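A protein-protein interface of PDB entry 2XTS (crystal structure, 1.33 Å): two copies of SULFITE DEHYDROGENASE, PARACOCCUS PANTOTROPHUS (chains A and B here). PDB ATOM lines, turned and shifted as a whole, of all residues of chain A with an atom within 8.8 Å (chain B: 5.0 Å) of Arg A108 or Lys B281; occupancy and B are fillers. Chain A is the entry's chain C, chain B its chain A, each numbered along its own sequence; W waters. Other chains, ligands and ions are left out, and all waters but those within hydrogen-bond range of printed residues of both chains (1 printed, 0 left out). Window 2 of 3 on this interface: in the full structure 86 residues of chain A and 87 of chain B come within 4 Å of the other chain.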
ATOM      1  N   PHE A 101     -13.478  -6.925   7.722  1.00  0.00           N
ATOM      2  CA  PHE A 101     -13.240  -7.761   8.874  1.00  0.00           C
ATOM      3  C   PHE A 101     -14.301  -8.823   9.025  1.00  0.00           C
ATOM      4  O   PHE A 101     -15.488  -8.587   8.791  1.00  0.00           O
ATOM      5  CB  PHE A 101     -13.274  -6.936  10.161  1.00  0.00           C
ATOM      6  CG  PHE A 101     -12.254  -5.839  10.219  1.00  0.00           C
ATOM      7  CD1 PHE A 101     -10.944  -6.117  10.530  1.00  0.00           C
ATOM      8  CD2 PHE A 101     -12.611  -4.527   9.987  1.00  0.00           C
ATOM      9  CE1 PHE A 101     -10.013  -5.109  10.607  1.00  0.00           C
ATOM     10  CE2 PHE A 101     -11.678  -3.517  10.066  1.00  0.00           C
ATOM     11  CZ  PHE A 101     -10.369  -3.813  10.376  1.00  0.00           C
ATOM     12  N   THR A 102     -13.868  -9.988   9.473  1.00  0.00           N
ATOM     13  CA  THR A 102     -14.752 -11.015   9.985  1.00  0.00           C
ATOM     14  C   THR A 102     -14.929 -10.828  11.495  1.00  0.00           C
ATOM     15  O   THR A 102     -14.168 -10.091  12.147  1.00  0.00           O
ATOM     16  CB  THR A 102     -14.166 -12.417   9.736  1.00  0.00           C
ATOM     17  OG1 THR A 102     -12.938 -12.536  10.457  1.00  0.00           O
ATOM     18  CG2 THR A 102     -13.899 -12.655   8.242  1.00  0.00           C
ATOM     19  N   PHE A 103     -15.917 -11.529  12.061  1.00  0.00           N
ATOM     20  CA  PHE A 103     -16.088 -11.468  13.500  1.00  0.00           C
ATOM     21  C   PHE A 103     -14.833 -12.027  14.203  1.00  0.00           C
ATOM     22  O   PHE A 103     -14.391 -11.509  15.218  1.00  0.00           O
ATOM     23  CB  PHE A 103     -17.340 -12.177  13.968  1.00  0.00           C
ATOM     24  CG  PHE A 103     -17.705 -11.810  15.355  1.00  0.00           C
ATOM     25  CD1 PHE A 103     -17.350 -12.621  16.406  1.00  0.00           C
ATOM     26  CD2 PHE A 103     -18.311 -10.589  15.633  1.00  0.00           C
ATOM     27  CE1 PHE A 103     -17.633 -12.254  17.712  1.00  0.00           C
ATOM     28  CE2 PHE A 103     -18.578 -10.230  16.931  1.00  0.00           C
ATOM     29  CZ  PHE A 103     -18.245 -11.068  17.962  1.00  0.00           C
ATOM     30  N   GLU A 104     -14.272 -13.114  13.683  1.00  0.00           N
ATOM     31  CA  GLU A 104     -13.032 -13.681  14.218  1.00  0.00           C
ATOM     32  C   GLU A 104     -11.943 -12.624  14.335  1.00  0.00           C
ATOM     33  O   GLU A 104     -11.219 -12.565  15.324  1.00  0.00           O
ATOM     34  CB  GLU A 104     -12.586 -14.825  13.308  1.00  0.00           C
ATOM     35  CG  GLU A 104     -11.263 -15.478  13.627  1.00  0.00           C
ATOM     36  CD  GLU A 104     -10.981 -16.637  12.684  1.00  0.00           C
ATOM     37  OE1 GLU A 104     -10.807 -16.394  11.469  1.00  0.00           O
ATOM     38  OE2 GLU A 104     -10.940 -17.790  13.160  1.00  0.00           O
ATOM     39  N   ASP A 105     -11.812 -11.781  13.313  1.00  0.00           N
ATOM     40  CA  ASP A 105     -10.795 -10.728  13.338  1.00  0.00           C
ATOM     41  C   ASP A 105     -11.059  -9.746  14.489  1.00  0.00           C
ATOM     42  O   ASP A 105     -10.143  -9.293  15.175  1.00  0.00           O
ATOM     43  CB  ASP A 105     -10.824  -9.882  12.063  1.00  0.00           C
ATOM     44  CG  ASP A 105     -10.444 -10.632  10.802  1.00  0.00           C
ATOM     45  OD1 ASP A 105      -9.633 -11.579  10.854  1.00  0.00           O
ATOM     46  OD2 ASP A 105     -10.923 -10.198   9.725  1.00  0.00           O
ATOM     47  N   LEU A 106     -12.325  -9.368  14.644  1.00  0.00           N
ATOM     48  CA  LEU A 106     -12.702  -8.379  15.629  1.00  0.00           C
ATOM     49  C   LEU A 106     -12.408  -8.794  17.083  1.00  0.00           C
ATOM     50  O   LEU A 106     -12.130  -7.946  17.921  1.00  0.00           O
ATOM     51  CB  LEU A 106     -14.167  -7.998  15.443  1.00  0.00           C
ATOM     52  CG  LEU A 106     -14.470  -7.263  14.116  1.00  0.00           C
ATOM     53  CD1 LEU A 106     -15.952  -7.080  13.926  1.00  0.00           C
ATOM     54  CD2 LEU A 106     -13.753  -5.925  14.028  1.00  0.00           C
ATOM     55  N   LEU A 107     -12.474 -10.096  17.366  1.00  0.00           N
ATOM     56  CA  LEU A 107     -12.130 -10.652  18.654  1.00  0.00           C
ATOM     57  C   LEU A 107     -10.650 -10.596  18.961  1.00  0.00           C
ATOM     58  O   LEU A 107     -10.244 -10.956  20.058  1.00  0.00           O
ATOM     59  CB  LEU A 107     -12.589 -12.100  18.715  1.00  0.00           C
ATOM     60  CG  LEU A 107     -14.092 -12.305  18.782  1.00  0.00           C
ATOM     61  CD1 LEU A 107     -14.437 -13.788  18.709  1.00  0.00           C
ATOM     62  CD2 LEU A 107     -14.677 -11.674  20.049  1.00  0.00           C
ATOM     63  N   ARG A 108      -9.843 -10.095  18.024  1.00  0.00           N
ATOM     64  CA  ARG A 108      -8.386 -10.036  18.204  1.00  0.00           C
ATOM     65  C   ARG A 108      -7.844  -8.648  18.490  1.00  0.00           C
ATOM     66  O   ARG A 108      -6.655  -8.484  18.764  1.00  0.00           O
ATOM     67  CB  ARG A 108      -7.691 -10.621  16.996  1.00  0.00           C
ATOM     68  CG  ARG A 108      -8.155 -12.024  16.674  1.00  0.00           C
ATOM     69  CD  ARG A 108      -7.548 -12.514  15.385  1.00  0.00           C
ATOM     70  NE  ARG A 108      -6.122 -12.716  15.532  1.00  0.00           N
ATOM     71  CZ  ARG A 108      -5.329 -13.190  14.580  1.00  0.00           C
ATOM     72  NH1 ARG A 108      -5.814 -13.494  13.388  1.00  0.00           N
ATOM     73  NH2 ARG A 108      -4.045 -13.341  14.834  1.00  0.00           N
ATOM     74  N   PHE A 109      -8.708  -7.634  18.404  1.00  0.00           N
ATOM     75  CA  PHE A 109      -8.296  -6.269  18.748  1.00  0.00           C
ATOM     76  C   PHE A 109      -8.336  -6.009  20.257  1.00  0.00           C
ATOM     77  O   PHE A 109      -9.153  -6.589  20.969  1.00  0.00           O
ATOM     78  CB  PHE A 109      -9.213  -5.243  18.079  1.00  0.00           C
ATOM     79  CG  PHE A 109      -8.957  -5.021  16.621  1.00  0.00           C
ATOM     80  CD1 PHE A 109      -8.052  -4.073  16.173  1.00  0.00           C
ATOM     81  CD2 PHE A 109      -9.680  -5.722  15.674  1.00  0.00           C
ATOM     82  CE1 PHE A 109      -7.874  -3.860  14.795  1.00  0.00           C
ATOM     83  CE2 PHE A 109      -9.481  -5.512  14.324  1.00  0.00           C
ATOM     84  CZ  PHE A 109      -8.595  -4.586  13.893  1.00  0.00           C
ATOM     85  N   PRO A 110      -7.541  -5.035  20.732  1.00  0.00           N
ATOM     86  CA  PRO A 110      -7.573  -4.646  22.146  1.00  0.00           C
ATOM     87  C   PRO A 110      -8.966  -4.191  22.563  1.00  0.00           C
ATOM     88  O   PRO A 110      -9.614  -3.439  21.841  1.00  0.00           O
ATOM     89  CB  PRO A 110      -6.549  -3.505  22.227  1.00  0.00           C
ATOM     90  CG  PRO A 110      -5.600  -3.805  21.140  1.00  0.00           C
ATOM     91  CD  PRO A 110      -6.405  -4.424  20.021  1.00  0.00           C
ATOM     92  N   ARG A 111      -9.406  -4.651  23.722  1.00  0.00           N
ATOM     93  CA  ARG A 111     -10.759  -4.424  24.179  1.00  0.00           C
ATOM     94  C   ARG A 111     -10.839  -3.333  25.232  1.00  0.00           C
ATOM     95  O   ARG A 111      -9.915  -3.106  26.009  1.00  0.00           O
ATOM     96  CB  ARG A 111     -11.310  -5.721  24.781  1.00  0.00           C
ATOM     97  CG  ARG A 111     -11.462  -6.847  23.764  1.00  0.00           C
ATOM     98  CD  ARG A 111     -11.959  -8.128  24.327  1.00  0.00           C
ATOM     99  NE  ARG A 111     -11.858  -9.145  23.293  1.00  0.00           N
ATOM    100  CZ  ARG A 111     -11.936 -10.445  23.494  1.00  0.00           C
ATOM    101  NH1 ARG A 111     -12.221 -10.923  24.697  1.00  0.00           N
ATOM    102  NH2 ARG A 111     -11.755 -11.273  22.480  1.00  0.00           N
ATOM    103  N   VAL A 151     -14.497  -3.042  21.187  1.00  0.00           N
ATOM    104  CA  VAL A 151     -13.277  -2.452  20.658  1.00  0.00           C
ATOM    105  C   VAL A 151     -13.546  -0.978  20.325  1.00  0.00           C
ATOM    106  O   VAL A 151     -14.553  -0.660  19.728  1.00  0.00           O
ATOM    107  CB  VAL A 151     -12.838  -3.220  19.404  1.00  0.00           C
ATOM    108  CG1 VAL A 151     -11.683  -2.571  18.724  1.00  0.00           C
ATOM    109  CG2 VAL A 151     -12.528  -4.666  19.771  1.00  0.00           C
ATOM    110  N   VAL A 155      -9.292   2.230  17.262  1.00  0.00           N
ATOM    111  CA  VAL A 155      -8.350   1.186  16.904  1.00  0.00           C
ATOM    112  C   VAL A 155      -8.667   0.516  15.567  1.00  0.00           C
ATOM    113  O   VAL A 155      -7.759   0.168  14.806  1.00  0.00           O
ATOM    114  CB  VAL A 155      -8.120   0.159  18.035  1.00  0.00           C
ATOM    115  CG1 VAL A 155      -9.183  -0.894  18.062  1.00  0.00           C
ATOM    116  CG2 VAL A 155      -6.718  -0.503  17.848  1.00  0.00           C
ATOM    117  N   LEU A 156      -9.950   0.360  15.247  1.00  0.00           N
ATOM    118  CA  LEU A 156     -10.343  -0.176  13.944  1.00  0.00           C
ATOM    119  C   LEU A 156      -9.981   0.806  12.836  1.00  0.00           C
ATOM    120  O   LEU A 156      -9.459   0.438  11.776  1.00  0.00           O
ATOM    121  CB  LEU A 156     -11.844  -0.435  13.923  1.00  0.00           C
ATOM    122  CG  LEU A 156     -12.363  -1.436  14.952  1.00  0.00           C
ATOM    123  CD1 LEU A 156     -13.891  -1.572  14.840  1.00  0.00           C
ATOM    124  CD2 LEU A 156     -11.684  -2.787  14.799  1.00  0.00           C
ATOM    125  N   GLU A 159      -6.402   0.901  11.778  1.00  0.00           N
ATOM    126  CA  GLU A 159      -6.019  -0.187  10.894  1.00  0.00           C
ATOM    127  C   GLU A 159      -6.166   0.184   9.409  1.00  0.00           C
ATOM    128  O   GLU A 159      -5.317  -0.141   8.572  1.00  0.00           O
ATOM    129  CB  GLU A 159      -6.830  -1.436  11.237  1.00  0.00           C
ATOM    130  CG  GLU A 159      -6.191  -2.731  10.844  1.00  0.00           C
ATOM    131  CD  GLU A 159      -4.881  -3.069  11.571  1.00  0.00           C
ATOM    132  OE1 GLU A 159      -4.601  -2.566  12.706  1.00  0.00           O
ATOM    133  OE2 GLU A 159      -4.164  -3.888  10.978  1.00  0.00           O
ATOM    134  N   PHE A 196     -19.505  -6.004  21.462  1.00  0.00           N
ATOM    135  CA  PHE A 196     -19.913  -7.382  21.213  1.00  0.00           C
ATOM    136  C   PHE A 196     -20.584  -8.035  22.401  1.00  0.00           C
ATOM    137  O   PHE A 196     -21.384  -8.966  22.223  1.00  0.00           O
ATOM    138  CB  PHE A 196     -18.732  -8.302  20.872  1.00  0.00           C
ATOM    139  CG  PHE A 196     -17.680  -7.681  20.029  1.00  0.00           C
ATOM    140  CD1 PHE A 196     -18.011  -7.050  18.834  1.00  0.00           C
ATOM    141  CD2 PHE A 196     -16.356  -7.720  20.413  1.00  0.00           C
ATOM    142  CE1 PHE A 196     -17.032  -6.442  18.059  1.00  0.00           C
ATOM    143  CE2 PHE A 196     -15.377  -7.109  19.650  1.00  0.00           C
ATOM    144  CZ  PHE A 196     -15.716  -6.483  18.468  1.00  0.00           C
ATOM    145  N   HIS B 279      -7.422 -19.057  15.115  1.00  0.00           N
ATOM    146  CA  HIS B 279      -7.202 -18.025  14.116  1.00  0.00           C
ATOM    147  C   HIS B 279      -5.768 -17.838  13.669  1.00  0.00           C
ATOM    148  O   HIS B 279      -5.483 -16.958  12.847  1.00  0.00           O
ATOM    149  CB  HIS B 279      -7.787 -16.683  14.571  1.00  0.00           C
ATOM    150  CG  HIS B 279      -7.267 -16.187  15.885  1.00  0.00           C
ATOM    151  ND1 HIS B 279      -5.928 -15.987  16.158  1.00  0.00           N
ATOM    152  CD2 HIS B 279      -7.938 -15.756  16.977  1.00  0.00           C
ATOM    153  CE1 HIS B 279      -5.805 -15.505  17.384  1.00  0.00           C
ATOM    154  NE2 HIS B 279      -7.010 -15.352  17.896  1.00  0.00           N
ATOM    155  N   GLY B 280      -4.863 -18.668  14.177  1.00  0.00           N
ATOM    156  CA  GLY B 280      -3.487 -18.634  13.710  1.00  0.00           C
ATOM    157  C   GLY B 280      -2.626 -17.653  14.474  1.00  0.00           C
ATOM    158  O   GLY B 280      -3.000 -17.134  15.532  1.00  0.00           O
ATOM    159  N   LYS B 281      -1.443 -17.396  13.925  1.00  0.00           N
ATOM    160  CA  LYS B 281      -0.465 -16.515  14.550  1.00  0.00           C
ATOM    161  C   LYS B 281      -0.899 -15.052  14.475  1.00  0.00           C
ATOM    162  O   LYS B 281      -1.746 -14.722  13.648  1.00  0.00           O
ATOM    163  CB  LYS B 281       0.886 -16.680  13.860  1.00  0.00           C
ATOM    164  CG  LYS B 281       1.288 -18.133  13.754  1.00  0.00           C
ATOM    165  CD  LYS B 281       2.663 -18.269  13.191  1.00  0.00           C
ATOM    166  CE  LYS B 281       3.066 -19.721  13.088  1.00  0.00           C
ATOM    167  NZ  LYS B 281       2.287 -20.454  12.062  1.00  0.00           N
ATOM    168  N   GLY B 282      -0.347 -14.215  15.347  1.00  0.00           N
ATOM    169  CA  GLY B 282      -0.567 -12.780  15.302  1.00  0.00           C
ATOM    170  C   GLY B 282      -1.280 -12.298  16.560  1.00  0.00           C
ATOM    171  O   GLY B 282      -1.257 -12.954  17.605  1.00  0.00           O
ATOM    172  N   PRO B 283      -1.942 -11.140  16.473  1.00  0.00           N
ATOM    173  CA  PRO B 283      -2.648 -10.572  17.625  1.00  0.00           C
ATOM    174  C   PRO B 283      -3.555 -11.567  18.346  1.00  0.00           C
ATOM    175  O   PRO B 283      -4.344 -12.280  17.725  1.00  0.00           O
ATOM    176  CB  PRO B 283      -3.486  -9.469  16.996  1.00  0.00           C
ATOM    177  CG  PRO B 283      -2.675  -9.046  15.813  1.00  0.00           C
ATOM    178  CD  PRO B 283      -2.054 -10.287  15.277  1.00  0.00           C
ATOM    179  N   LEU B 284      -3.450 -11.572  19.665  1.00  0.00           N
ATOM    180  CA  LEU B 284      -4.215 -12.466  20.527  1.00  0.00           C
ATOM    181  C   LEU B 284      -4.581 -11.709  21.776  1.00  0.00           C
ATOM    182  O   LEU B 284      -3.708 -11.118  22.423  1.00  0.00           O
ATOM    183  CB  LEU B 284      -3.361 -13.685  20.898  1.00  0.00           C
ATOM    184  CG  LEU B 284      -3.983 -14.760  21.777  1.00  0.00           C
ATOM    185  CD1 LEU B 284      -5.105 -15.485  21.071  1.00  0.00           C
ATOM    186  CD2 LEU B 284      -2.920 -15.729  22.227  1.00  0.00           C
ATOM    187  N   VAL B 285      -5.870 -11.748  22.131  1.00  0.00           N
ATOM    188  CA  VAL B 285      -6.337 -11.184  23.394  1.00  0.00           C
ATOM    189  C   VAL B 285      -6.280 -12.245  24.492  1.00  0.00           C
ATOM    190  O   VAL B 285      -6.838 -13.333  24.361  1.00  0.00           O
ATOM    191  CB  VAL B 285      -7.784 -10.673  23.262  1.00  0.00           C
ATOM    192  CG1 VAL B 285      -8.325 -10.257  24.651  1.00  0.00           C
ATOM    193  CG2 VAL B 285      -7.853  -9.516  22.222  1.00  0.00           C
ATOM    194  N   TRP B 333       1.083 -13.481  19.106  1.00  0.00           N
ATOM    195  CA  TRP B 333       1.441 -14.899  19.253  1.00  0.00           C
ATOM    196  C   TRP B 333       2.213 -15.397  18.030  1.00  0.00           C
ATOM    197  O   TRP B 333       1.697 -15.366  16.907  1.00  0.00           O
ATOM    198  CB  TRP B 333       0.186 -15.741  19.489  1.00  0.00           C
ATOM    199  CG  TRP B 333       0.491 -17.195  19.783  1.00  0.00           C
ATOM    200  CD1 TRP B 333       1.463 -17.690  20.621  1.00  0.00           C
ATOM    201  CD2 TRP B 333      -0.172 -18.331  19.232  1.00  0.00           C
ATOM    202  NE1 TRP B 333       1.425 -19.056  20.627  1.00  0.00           N
ATOM    203  CE2 TRP B 333       0.426 -19.483  19.794  1.00  0.00           C
ATOM    204  CE3 TRP B 333      -1.223 -18.494  18.331  1.00  0.00           C
ATOM    205  CZ2 TRP B 333       0.020 -20.772  19.453  1.00  0.00           C
ATOM    206  CZ3 TRP B 333      -1.635 -19.757  18.008  1.00  0.00           C
ATOM    207  CH2 TRP B 333      -1.022 -20.891  18.572  1.00  0.00           C
ATOM    208  N   ASP B 334       3.449 -15.846  18.264  1.00  0.00           N
ATOM    209  CA  ASP B 334       4.304 -16.359  17.189  1.00  0.00           C
ATOM    210  C   ASP B 334       4.078 -17.857  16.899  1.00  0.00           C
ATOM    211  O   ASP B 334       4.777 -18.448  16.095  1.00  0.00           O
ATOM    212  CB  ASP B 334       5.791 -16.052  17.463  1.00  0.00           C
ATOM    213  CG  ASP B 334       6.328 -16.738  18.701  1.00  0.00           C
ATOM    214  OD1 ASP B 334       5.597 -17.535  19.318  1.00  0.00           O
ATOM    215  OD2 ASP B 334       7.510 -16.488  19.044  1.00  0.00           O
ATOM    216  N   GLY B 335       3.084 -18.476  17.540  1.00  0.00           N
ATOM    217  CA  GLY B 335       2.764 -19.865  17.286  1.00  0.00           C
ATOM    218  C   GLY B 335       3.528 -20.834  18.185  1.00  0.00           C
ATOM    219  O   GLY B 335       3.358 -22.028  18.060  1.00  0.00           O
HETATM  220  O   HOH W   1      -8.071 -12.825  20.511  1.00  0.00           O
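The guanidinium group of Arg A108 lies close to a ring nitrogen (ND1) of His B279 (3.3 Å).
The guanidinium group (NE) of Arg A108 lies within hydrogen-bond range of the backbone carbonyl oxygen (O) of Pro B283 (2.9 Å).
The backbone carbonyl oxygen (O) of Lys B281 is in hydrogen-bond range of the guanidinium group (NH2) of Arg A108.
The backbone carbonyl oxygen (O) of Trp B333 lies within hydrogen-bond range of the backbone NH (N) of Gly B282 (2.8 Å).
The backbone carbonyl oxygen of Leu A107 sits at hydrogen-bond distance from the guanidinium group of Arg A111 (2.9 Å).
Among the printed residues, merely in contact across the chains: Glu A104 with His B279 (3.6 Å), Leu A107 with Val B285 (3.5 Å), Arg A108 with Gly B280 (3.996 Å), Arg A108 with Gly B282 (3.4 Å), Arg A108 with Val B285 (3.8 Å), Phe A109 with Val B285 (3.4 Å) and Arg A111 with Val B285 (3.8 Å).
Of the printed residues of chain B, Arg A108 touches His B279, Gly B280, Lys B281, Gly B282, Pro B283 and Val B285.
Lys B281 touches one residue of chain A.
Printed residues of chain A within 4 Å of Pro B283: Arg A108 (2.9 Å).
Of the printed residues of chain B, Glu A104 touches His B279.
Of the printed residues of chain B, Phe A109 touches Val B285 (3.4 Å).
The nearest printed residue of chain A that does not touch His B279 is Leu A107 (5.9 Å).
Of the 10 printed residues of chain B, 6 touch a printed residue of chain A.
Of the 16 printed residues of chain A, 5 touch a printed residue of chain B.
No position is printed for both chains.
Water W1 lies within hydrogen-bond range of the backbone carbonyl oxygen of Leu A107 (2.9 Å) and the backbone NH of Val B285 (2.9 Å).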
